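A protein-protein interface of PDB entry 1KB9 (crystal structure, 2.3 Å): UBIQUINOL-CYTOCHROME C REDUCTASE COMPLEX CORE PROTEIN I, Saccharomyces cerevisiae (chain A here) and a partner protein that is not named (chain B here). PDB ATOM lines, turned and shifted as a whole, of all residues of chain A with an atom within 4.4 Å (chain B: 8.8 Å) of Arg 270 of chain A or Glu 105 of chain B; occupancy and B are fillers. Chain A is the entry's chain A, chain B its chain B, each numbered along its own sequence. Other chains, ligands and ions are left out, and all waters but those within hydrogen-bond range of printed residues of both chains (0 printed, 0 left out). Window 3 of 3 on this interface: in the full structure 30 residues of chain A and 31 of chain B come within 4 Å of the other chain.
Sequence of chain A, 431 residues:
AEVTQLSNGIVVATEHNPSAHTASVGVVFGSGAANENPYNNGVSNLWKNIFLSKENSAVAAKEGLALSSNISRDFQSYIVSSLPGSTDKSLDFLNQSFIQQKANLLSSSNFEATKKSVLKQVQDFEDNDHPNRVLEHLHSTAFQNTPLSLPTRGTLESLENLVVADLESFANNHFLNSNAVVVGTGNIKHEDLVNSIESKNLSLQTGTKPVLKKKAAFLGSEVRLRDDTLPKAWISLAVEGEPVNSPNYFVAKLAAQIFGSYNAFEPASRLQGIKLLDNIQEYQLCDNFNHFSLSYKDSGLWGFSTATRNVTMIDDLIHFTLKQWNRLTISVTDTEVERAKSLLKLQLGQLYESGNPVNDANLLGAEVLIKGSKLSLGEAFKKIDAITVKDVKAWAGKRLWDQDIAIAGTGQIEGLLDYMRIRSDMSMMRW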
ATOM      1  N   TYR A 262     -20.450  -3.702  37.906  1.00  0.00           N
ATOM      2  CA  TYR A 262     -19.422  -3.593  36.887  1.00  0.00           C
ATOM      3  C   TYR A 262     -19.729  -4.411  35.645  1.00  0.00           C
ATOM      4  O   TYR A 262     -20.413  -5.421  35.712  1.00  0.00           O
ATOM      5  CB  TYR A 262     -18.082  -4.016  37.511  1.00  0.00           C
ATOM      6  CG  TYR A 262     -16.948  -4.293  36.546  1.00  0.00           C
ATOM      7  CD1 TYR A 262     -16.586  -5.604  36.228  1.00  0.00           C
ATOM      8  CD2 TYR A 262     -16.211  -3.254  35.983  1.00  0.00           C
ATOM      9  CE1 TYR A 262     -15.518  -5.872  35.376  1.00  0.00           C
ATOM     10  CE2 TYR A 262     -15.139  -3.513  35.132  1.00  0.00           C
ATOM     11  CZ  TYR A 262     -14.801  -4.825  34.835  1.00  0.00           C
ATOM     12  OH  TYR A 262     -13.748  -5.086  33.991  1.00  0.00           O
ATOM     13  N   ALA A 264     -17.285  -5.438  32.368  1.00  0.00           N
ATOM     14  CA  ALA A 264     -15.992  -5.400  31.699  1.00  0.00           C
ATOM     15  C   ALA A 264     -15.996  -4.935  30.252  1.00  0.00           C
ATOM     16  O   ALA A 264     -14.962  -4.525  29.735  1.00  0.00           O
ATOM     17  CB  ALA A 264     -15.330  -6.766  31.790  1.00  0.00           C
ATOM     18  N   GLU A 266     -18.074  -2.460  28.969  1.00  0.00           N
ATOM     19  CA  GLU A 266     -18.443  -1.050  28.898  1.00  0.00           C
ATOM     20  C   GLU A 266     -17.276  -0.174  29.364  1.00  0.00           C
ATOM     21  O   GLU A 266     -16.956  -0.125  30.554  1.00  0.00           O
ATOM     22  CB  GLU A 266     -19.690  -0.775  29.757  1.00  0.00           C
ATOM     23  CG  GLU A 266     -21.013  -1.207  29.125  1.00  0.00           C
ATOM     24  CD  GLU A 266     -21.337  -0.451  27.832  1.00  0.00           C
ATOM     25  OE1 GLU A 266     -21.846  -1.082  26.880  1.00  0.00           O
ATOM     26  OE2 GLU A 266     -21.083   0.774  27.767  1.00  0.00           O
ATOM     27  N   PRO A 267     -16.632   0.537  28.424  1.00  0.00           N
ATOM     28  CA  PRO A 267     -15.494   1.426  28.686  1.00  0.00           C
ATOM     29  C   PRO A 267     -15.631   2.289  29.944  1.00  0.00           C
ATOM     30  O   PRO A 267     -14.715   2.354  30.772  1.00  0.00           O
ATOM     31  CB  PRO A 267     -15.446   2.272  27.421  1.00  0.00           C
ATOM     32  CG  PRO A 267     -15.814   1.270  26.360  1.00  0.00           C
ATOM     33  CD  PRO A 267     -16.999   0.568  26.994  1.00  0.00           C
ATOM     34  N   ALA A 268     -16.795   2.907  30.106  1.00  0.00           N
ATOM     35  CA  ALA A 268     -17.058   3.772  31.255  1.00  0.00           C
ATOM     36  C   ALA A 268     -17.082   3.036  32.580  1.00  0.00           C
ATOM     37  O   ALA A 268     -16.742   3.609  33.614  1.00  0.00           O
ATOM     38  CB  ALA A 268     -18.374   4.519  31.062  1.00  0.00           C
ATOM     39  N   SER A 269     -17.521   1.783  32.559  1.00  0.00           N
ATOM     40  CA  SER A 269     -17.609   0.983  33.782  1.00  0.00           C
ATOM     41  C   SER A 269     -16.226   0.664  34.344  1.00  0.00           C
ATOM     42  O   SER A 269     -16.036   0.597  35.562  1.00  0.00           O
ATOM     43  CB  SER A 269     -18.386  -0.310  33.520  1.00  0.00           C
ATOM     44  OG  SER A 269     -18.777  -0.931  34.734  1.00  0.00           O
ATOM     45  N   ARG A 270     -15.261   0.506  33.445  1.00  0.00           N
ATOM     46  CA  ARG A 270     -13.884   0.199  33.816  1.00  0.00           C
ATOM     47  C   ARG A 270     -13.187   1.397  34.465  1.00  0.00           C
ATOM     48  O   ARG A 270     -12.103   1.257  35.032  1.00  0.00           O
ATOM     49  CB  ARG A 270     -13.097  -0.246  32.575  1.00  0.00           C
ATOM     50  CG  ARG A 270     -13.799  -1.319  31.745  1.00  0.00           C
ATOM     51  CD  ARG A 270     -12.834  -2.102  30.869  1.00  0.00           C
ATOM     52  NE  ARG A 270     -12.360  -1.332  29.726  1.00  0.00           N
ATOM     53  CZ  ARG A 270     -12.408  -1.753  28.461  1.00  0.00           C
ATOM     54  NH1 ARG A 270     -11.951  -0.976  27.479  1.00  0.00           N
ATOM     55  NH2 ARG A 270     -12.915  -2.948  28.168  1.00  0.00           N
ATOM     56  N   LEU A 271     -13.825   2.568  34.404  1.00  0.00           N
ATOM     57  CA  LEU A 271     -13.238   3.790  34.950  1.00  0.00           C
ATOM     58  C   LEU A 271     -13.783   4.251  36.299  1.00  0.00           C
ATOM     59  O   LEU A 271     -13.292   5.219  36.865  1.00  0.00           O
ATOM     60  CB  LEU A 271     -13.364   4.917  33.928  1.00  0.00           C
ATOM     61  CG  LEU A 271     -12.813   4.626  32.529  1.00  0.00           C
ATOM     62  CD1 LEU A 271     -13.261   5.712  31.538  1.00  0.00           C
ATOM     63  CD2 LEU A 271     -11.291   4.515  32.576  1.00  0.00           C
ATOM     64  N   GLN A 272     -14.772   3.549  36.832  1.00  0.00           N
ATOM     65  CA  GLN A 272     -15.358   3.934  38.112  1.00  0.00           C
ATOM     66  C   GLN A 272     -14.390   4.016  39.287  1.00  0.00           C
ATOM     67  O   GLN A 272     -13.395   3.278  39.354  1.00  0.00           O
ATOM     68  CB  GLN A 272     -16.484   2.983  38.483  1.00  0.00           C
ATOM     69  CG  GLN A 272     -17.576   2.874  37.454  1.00  0.00           C
ATOM     70  CD  GLN A 272     -18.590   1.839  37.851  1.00  0.00           C
ATOM     71  OE1 GLN A 272     -19.293   2.002  38.853  1.00  0.00           O
ATOM     72  NE2 GLN A 272     -18.637   0.737  37.106  1.00  0.00           N
ATOM     73  N   LEU A 277     -11.602  -2.567  41.343  1.00  0.00           N
ATOM     74  CA  LEU A 277     -11.344  -2.649  39.904  1.00  0.00           C
ATOM     75  C   LEU A 277      -9.879  -2.736  39.514  1.00  0.00           C
ATOM     76  O   LEU A 277      -9.554  -3.223  38.429  1.00  0.00           O
ATOM     77  CB  LEU A 277     -12.005  -1.491  39.158  1.00  0.00           C
ATOM     78  CG  LEU A 277     -13.530  -1.470  39.185  1.00  0.00           C
ATOM     79  CD1 LEU A 277     -14.017  -0.408  38.210  1.00  0.00           C
ATOM     80  CD2 LEU A 277     -14.090  -2.837  38.807  1.00  0.00           C
ATOM     81  N   GLN A 281      -9.175  -6.189  37.061  1.00  0.00           N
ATOM     82  CA  GLN A 281      -8.951  -5.931  35.642  1.00  0.00           C
ATOM     83  C   GLN A 281      -7.632  -6.417  35.068  1.00  0.00           C
ATOM     84  O   GLN A 281      -7.536  -6.646  33.863  1.00  0.00           O
ATOM     85  CB  GLN A 281      -9.151  -4.455  35.323  1.00  0.00           C
ATOM     86  CG  GLN A 281     -10.530  -3.966  35.712  1.00  0.00           C
ATOM     87  CD  GLN A 281     -10.934  -2.714  34.979  1.00  0.00           C
ATOM     88  OE1 GLN A 281     -11.705  -2.773  34.021  1.00  0.00           O
ATOM     89  NE2 GLN A 281     -10.416  -1.573  35.417  1.00  0.00           N
ATOM     90  N   PHE B  38     -17.431   6.275  20.434  1.00  0.00           N
ATOM     91  CA  PHE B  38     -16.356   7.227  20.718  1.00  0.00           C
ATOM     92  C   PHE B  38     -16.779   8.353  21.662  1.00  0.00           C
ATOM     93  O   PHE B  38     -15.926   9.045  22.223  1.00  0.00           O
ATOM     94  CB  PHE B  38     -15.818   7.835  19.418  1.00  0.00           C
ATOM     95  CG  PHE B  38     -14.322   7.758  19.281  1.00  0.00           C
ATOM     96  CD1 PHE B  38     -13.747   7.179  18.152  1.00  0.00           C
ATOM     97  CD2 PHE B  38     -13.484   8.258  20.285  1.00  0.00           C
ATOM     98  CE1 PHE B  38     -12.357   7.096  18.018  1.00  0.00           C
ATOM     99  CE2 PHE B  38     -12.094   8.179  20.162  1.00  0.00           C
ATOM    100  CZ  PHE B  38     -11.529   7.596  19.025  1.00  0.00           C
ATOM    101  N   GLN B  41     -15.248   9.650  25.450  1.00  0.00           N
ATOM    102  CA  GLN B  41     -13.858   9.236  25.527  1.00  0.00           C
ATOM    103  C   GLN B  41     -13.117  10.506  25.949  1.00  0.00           C
ATOM    104  O   GLN B  41     -13.684  11.356  26.644  1.00  0.00           O
ATOM    105  CB  GLN B  41     -13.352   8.749  24.170  1.00  0.00           C
ATOM    106  CG  GLN B  41     -13.762   7.322  23.825  1.00  0.00           C
ATOM    107  CD  GLN B  41     -13.201   6.286  24.796  1.00  0.00           C
ATOM    108  OE1 GLN B  41     -13.900   5.362  25.199  1.00  0.00           O
ATOM    109  NE2 GLN B  41     -11.934   6.436  25.164  1.00  0.00           N
ATOM    110  N   ALA B  48     -11.551  10.852  29.737  1.00  0.00           N
ATOM    111  CA  ALA B  48     -12.697   9.986  30.007  1.00  0.00           C
ATOM    112  C   ALA B  48     -12.707   9.591  31.482  1.00  0.00           C
ATOM    113  O   ALA B  48     -13.753   9.584  32.127  1.00  0.00           O
ATOM    114  CB  ALA B  48     -12.638   8.744  29.119  1.00  0.00           C
ATOM    115  N   LEU B  49     -11.523   9.315  32.022  1.00  0.00           N
ATOM    116  CA  LEU B  49     -11.390   8.936  33.422  1.00  0.00           C
ATOM    117  C   LEU B  49     -11.897  10.036  34.364  1.00  0.00           C
ATOM    118  O   LEU B  49     -12.754   9.786  35.214  1.00  0.00           O
ATOM    119  CB  LEU B  49      -9.928   8.593  33.742  1.00  0.00           C
ATOM    120  CG  LEU B  49      -9.531   8.416  35.210  1.00  0.00           C
ATOM    121  CD1 LEU B  49     -10.196   7.189  35.811  1.00  0.00           C
ATOM    122  CD2 LEU B  49      -8.023   8.306  35.307  1.00  0.00           C
ATOM    123  N   VAL B  52     -15.751  10.682  34.439  1.00  0.00           N
ATOM    124  CA  VAL B  52     -16.434   9.684  35.252  1.00  0.00           C
ATOM    125  C   VAL B  52     -16.195   9.951  36.736  1.00  0.00           C
ATOM    126  O   VAL B  52     -17.128  10.003  37.534  1.00  0.00           O
ATOM    127  CB  VAL B  52     -15.942   8.253  34.901  1.00  0.00           C
ATOM    128  CG1 VAL B  52     -16.558   7.225  35.835  1.00  0.00           C
ATOM    129  CG2 VAL B  52     -16.269   7.917  33.457  1.00  0.00           C
ATOM    130  N   ARG B  53     -14.942  10.159  37.106  1.00  0.00           N
ATOM    131  CA  ARG B  53     -14.629  10.399  38.506  1.00  0.00           C
ATOM    132  C   ARG B  53     -15.339  11.630  39.050  1.00  0.00           C
ATOM    133  O   ARG B  53     -15.837  11.602  40.169  1.00  0.00           O
ATOM    134  CB  ARG B  53     -13.116  10.484  38.711  1.00  0.00           C
ATOM    135  CG  ARG B  53     -12.377   9.316  38.073  1.00  0.00           C
ATOM    136  CD  ARG B  53     -12.841   7.977  38.632  1.00  0.00           C
ATOM    137  NE  ARG B  53     -12.168   7.703  39.889  1.00  0.00           N
ATOM    138  CZ  ARG B  53     -11.194   6.812  40.040  1.00  0.00           C
ATOM    139  NH1 ARG B  53     -10.626   6.666  41.225  1.00  0.00           N
ATOM    140  NH2 ARG B  53     -10.838   6.021  39.034  1.00  0.00           N
ATOM    141  N   GLU B  56     -19.310  11.112  39.168  1.00  0.00           N
ATOM    142  CA  GLU B  56     -19.676  10.199  40.250  1.00  0.00           C
ATOM    143  C   GLU B  56     -19.793  10.938  41.575  1.00  0.00           C
ATOM    144  O   GLU B  56     -20.714  10.687  42.349  1.00  0.00           O
ATOM    145  CB  GLU B  56     -18.656   9.061  40.392  1.00  0.00           C
ATOM    146  CG  GLU B  56     -18.622   8.078  39.225  1.00  0.00           C
ATOM    147  CD  GLU B  56     -17.752   6.844  39.482  1.00  0.00           C
ATOM    148  OE1 GLU B  56     -16.866   6.870  40.365  1.00  0.00           O
ATOM    149  OE2 GLU B  56     -17.973   5.833  38.792  1.00  0.00           O
ATOM    150  N   LYS B  99      -7.942  10.151  19.715  1.00  0.00           N
ATOM    151  CA  LYS B  99      -6.583   9.606  19.683  1.00  0.00           C
ATOM    152  C   LYS B  99      -6.593   8.205  19.067  1.00  0.00           C
ATOM    153  O   LYS B  99      -7.488   7.414  19.342  1.00  0.00           O
ATOM    154  CB  LYS B  99      -5.999   9.548  21.098  1.00  0.00           C
ATOM    155  CG  LYS B  99      -5.911  10.904  21.799  1.00  0.00           C
ATOM    156  CD  LYS B  99      -4.975  11.855  21.064  1.00  0.00           C
ATOM    157  CE  LYS B  99      -3.650  12.018  21.790  1.00  0.00           C
ATOM    158  NZ  LYS B  99      -3.821  12.746  23.082  1.00  0.00           N
ATOM    159  N   PRO B 100      -5.588   7.882  18.235  1.00  0.00           N
ATOM    160  CA  PRO B 100      -5.488   6.568  17.581  1.00  0.00           C
ATOM    161  C   PRO B 100      -5.517   5.388  18.558  1.00  0.00           C
ATOM    162  O   PRO B 100      -6.065   4.330  18.246  1.00  0.00           O
ATOM    163  CB  PRO B 100      -4.137   6.644  16.859  1.00  0.00           C
ATOM    164  CG  PRO B 100      -3.981   8.097  16.573  1.00  0.00           C
ATOM    165  CD  PRO B 100      -4.448   8.736  17.861  1.00  0.00           C
ATOM    166  N   HIS B 101      -4.933   5.573  19.741  1.00  0.00           N
ATOM    167  CA  HIS B 101      -4.898   4.508  20.729  1.00  0.00           C
ATOM    168  C   HIS B 101      -6.243   4.303  21.405  1.00  0.00           C
ATOM    169  O   HIS B 101      -6.517   3.222  21.927  1.00  0.00           O
ATOM    170  CB  HIS B 101      -3.796   4.739  21.764  1.00  0.00           C
ATOM    171  CG  HIS B 101      -4.083   5.835  22.743  1.00  0.00           C
ATOM    172  ND1 HIS B 101      -3.477   7.071  22.672  1.00  0.00           N
ATOM    173  CD2 HIS B 101      -4.857   5.859  23.853  1.00  0.00           C
ATOM    174  CE1 HIS B 101      -3.861   7.806  23.701  1.00  0.00           C
ATOM    175  NE2 HIS B 101      -4.698   7.095  24.433  1.00  0.00           N
ATOM    176  N   GLU B 102      -7.066   5.351  21.425  1.00  0.00           N
ATOM    177  CA  GLU B 102      -8.396   5.252  22.021  1.00  0.00           C
ATOM    178  C   GLU B 102      -9.249   4.397  21.104  1.00  0.00           C
ATOM    179  O   GLU B 102     -10.126   3.670  21.555  1.00  0.00           O
ATOM    180  CB  GLU B 102      -9.035   6.626  22.178  1.00  0.00           C
ATOM    181  CG  GLU B 102      -8.314   7.522  23.150  1.00  0.00           C
ATOM    182  CD  GLU B 102      -9.139   8.725  23.525  1.00  0.00           C
ATOM    183  OE1 GLU B 102      -9.144   9.709  22.753  1.00  0.00           O
ATOM    184  OE2 GLU B 102      -9.793   8.678  24.587  1.00  0.00           O
ATOM    185  N   LEU B 103      -8.962   4.478  19.810  1.00  0.00           N
ATOM    186  CA  LEU B 103      -9.689   3.703  18.826  1.00  0.00           C
ATOM    187  C   LEU B 103      -9.429   2.218  19.053  1.00  0.00           C
ATOM    188  O   LEU B 103     -10.359   1.451  19.323  1.00  0.00           O
ATOM    189  CB  LEU B 103      -9.261   4.103  17.408  1.00  0.00           C
ATOM    190  CG  LEU B 103      -9.901   3.314  16.260  1.00  0.00           C
ATOM    191  CD1 LEU B 103     -11.421   3.411  16.342  1.00  0.00           C
ATOM    192  CD2 LEU B 103      -9.390   3.822  14.916  1.00  0.00           C
ATOM    193  N   THR B 104      -8.152   1.841  19.004  1.00  0.00           N
ATOM    194  CA  THR B 104      -7.728   0.450  19.171  1.00  0.00           C
ATOM    195  C   THR B 104      -7.955  -0.188  20.544  1.00  0.00           C
ATOM    196  O   THR B 104      -8.247  -1.378  20.631  1.00  0.00           O
ATOM    197  CB  THR B 104      -6.241   0.286  18.809  1.00  0.00           C
ATOM    198  OG1 THR B 104      -5.455   1.142  19.642  1.00  0.00           O
ATOM    199  CG2 THR B 104      -5.993   0.653  17.358  1.00  0.00           C
ATOM    200  N   GLU B 105      -7.855   0.603  21.604  1.00  0.00           N
ATOM    201  CA  GLU B 105      -8.009   0.089  22.960  1.00  0.00           C
ATOM    202  C   GLU B 105      -9.396   0.127  23.590  1.00  0.00           C
ATOM    203  O   GLU B 105      -9.677  -0.677  24.477  1.00  0.00           O
ATOM    204  CB  GLU B 105      -7.028   0.794  23.906  1.00  0.00           C
ATOM    205  CG  GLU B 105      -5.568   0.642  23.528  1.00  0.00           C
ATOM    206  CD  GLU B 105      -4.636   1.446  24.419  1.00  0.00           C
ATOM    207  OE1 GLU B 105      -5.100   2.021  25.435  1.00  0.00           O
ATOM    208  OE2 GLU B 105      -3.431   1.503  24.097  1.00  0.00           O
ATOM    209  N   SER B 106     -10.250   1.056  23.165  1.00  0.00           N
ATOM    210  CA  SER B 106     -11.587   1.167  23.758  1.00  0.00           C
ATOM    211  C   SER B 106     -12.770   1.150  22.805  1.00  0.00           C
ATOM    212  O   SER B 106     -13.794   0.538  23.105  1.00  0.00           O
ATOM    213  CB  SER B 106     -11.687   2.425  24.619  1.00  0.00           C
ATOM    214  OG  SER B 106     -10.697   2.436  25.630  1.00  0.00           O
ATOM    215  N   VAL B 107     -12.640   1.844  21.677  1.00  0.00           N
ATOM    216  CA  VAL B 107     -13.723   1.937  20.701  1.00  0.00           C
ATOM    217  C   VAL B 107     -13.964   0.662  19.904  1.00  0.00           C
ATOM    218  O   VAL B 107     -15.087   0.150  19.877  1.00  0.00           O
ATOM    219  CB  VAL B 107     -13.512   3.146  19.753  1.00  0.00           C
ATOM    220  CG1 VAL B 107     -14.614   3.208  18.696  1.00  0.00           C
ATOM    221  CG2 VAL B 107     -13.497   4.432  20.564  1.00  0.00           C
ATOM    222  N   LEU B 108     -12.924   0.151  19.254  1.00  0.00           N
ATOM    223  CA  LEU B 108     -13.058  -1.073  18.474  1.00  0.00           C
ATOM    224  C   LEU B 108     -13.527  -2.269  19.317  1.00  0.00           C
ATOM    225  O   LEU B 108     -14.407  -3.010  18.893  1.00  0.00           O
ATOM    226  CB  LEU B 108     -11.758  -1.392  17.729  1.00  0.00           C
ATOM    227  CG  LEU B 108     -11.439  -0.438  16.573  1.00  0.00           C
ATOM    228  CD1 LEU B 108     -10.157  -0.864  15.852  1.00  0.00           C
ATOM    229  CD2 LEU B 108     -12.614  -0.417  15.594  1.00  0.00           C
ATOM    230  N   PRO B 109     -12.935  -2.482  20.510  1.00  0.00           N
ATOM    231  CA  PRO B 109     -13.364  -3.610  21.348  1.00  0.00           C
ATOM    232  C   PRO B 109     -14.829  -3.489  21.753  1.00  0.00           C
ATOM    233  O   PRO B 109     -15.590  -4.447  21.632  1.00  0.00           O
ATOM    234  CB  PRO B 109     -12.443  -3.495  22.565  1.00  0.00           C
ATOM    235  CG  PRO B 109     -11.191  -2.978  21.961  1.00  0.00           C
ATOM    236  CD  PRO B 109     -11.702  -1.884  21.056  1.00  0.00           C
ATOM    237  N   ALA B 110     -15.223  -2.304  22.214  1.00  0.00           N
ATOM    238  CA  ALA B 110     -16.603  -2.057  22.636  1.00  0.00           C
ATOM    239  C   ALA B 110     -17.580  -2.272  21.490  1.00  0.00           C
ATOM    240  O   ALA B 110     -18.673  -2.792  21.693  1.00  0.00           O
ATOM    241  CB  ALA B 110     -16.746  -0.653  23.194  1.00  0.00           C
ATOM    242  N   ALA B 111     -17.170  -1.887  20.285  1.00  0.00           N
ATOM    243  CA  ALA B 111     -17.999  -2.047  19.097  1.00  0.00           C
ATOM    244  C   ALA B 111     -18.078  -3.509  18.668  1.00  0.00           C
ATOM    245  O   ALA B 111     -19.116  -3.955  18.179  1.00  0.00           O
ATOM    246  CB  ALA B 111     -17.455  -1.198  17.959  1.00  0.00           C
ATOM    247  N   TYR B 113     -17.954  -6.058  20.620  1.00  0.00           N
ATOM    248  CA  TYR B 113     -18.828  -6.687  21.603  1.00  0.00           C
ATOM    249  C   TYR B 113     -20.288  -6.406  21.245  1.00  0.00           C
ATOM    250  O   TYR B 113     -21.140  -7.291  21.349  1.00  0.00           O
ATOM    251  CB  TYR B 113     -18.467  -6.171  23.003  1.00  0.00           C
ATOM    252  CG  TYR B 113     -19.587  -6.107  24.024  1.00  0.00           C
ATOM    253  CD1 TYR B 113     -20.072  -7.258  24.651  1.00  0.00           C
ATOM    254  CD2 TYR B 113     -20.109  -4.872  24.419  1.00  0.00           C
ATOM    255  CE1 TYR B 113     -21.049  -7.179  25.653  1.00  0.00           C
ATOM    256  CE2 TYR B 113     -21.082  -4.780  25.417  1.00  0.00           C
ATOM    257  CZ  TYR B 113     -21.547  -5.932  26.033  1.00  0.00           C
ATOM    258  OH  TYR B 113     -22.494  -5.812  27.036  1.00  0.00           O
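NH2 of Arg 53 of chain B lies close to O of Leu 271 of chain A, at 3.4 Å.
NH2 of Arg 270 of chain A lies within hydrogen-bond range of O of Ala 264 of chain A, 3.0 Å away. The side-chain hydroxyl (OG) of Ser 269 of chain A lies within hydrogen-bond range of the side-chain amide nitrogen (NE2) of Gln 272 of chain A, 2.9 Å away. The backbone carbonyl oxygen (O) of Arg 270 of chain A is in hydrogen-bond range of the side-chain amide nitrogen (NE2) of Gln 281 of chain A.
Among the printed residues, pairs that only touch across the chains: Pro 267 of chain A with Ser 106 of chain B (3.9 Å), Pro 267 of chain A with Ala 110 of chain B (3.8 Å), Arg 270 of chain A with Glu 105 of chain B (3.8 Å), Leu 271 of chain A with Ala 48 of chain B (3.9 Å), Leu 271 of chain A with Leu 49 of chain B (3.8 Å), Leu 271 of chain A with Val 52 of chain B (3.97 Å), Gln 272 of chain A with Arg 53 of chain B (3.8 Å) and Gln 272 of chain A with Glu 56 of chain B (3.2 Å).
Of the printed residues of chain B, Arg 270 of chain A touches Glu 105. Of chain A, only Arg 270 (3.8 Å) comes within 4 Å of Glu 105 of chain B. Of the printed residues of chain A, Leu 49 of chain B touches Leu 271. Of the printed residues of chain A, Ser 106 of chain B touches Pro 267 (3.9 Å). The nearest printed residue of chain A that does not touch Ser 106 of chain B is Arg 270 of chain A (4.1 Å).
Of the 21 printed residues of chain B, 8 touch a printed residue of chain A. Hydrophobic or aromatic side chains of chain B within 4 Å of the printed part of chain A: Ala 48, Leu 49, Val 52 and Ala 110. Hydrophobic or aromatic side chains of chain A that line the printed part of chain B: Pro 267 and Leu 271. Among the printed residues, no Asp or Glu carboxylate lies within 4 Å of a Lys or Arg side-chain nitrogen of the other chain.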
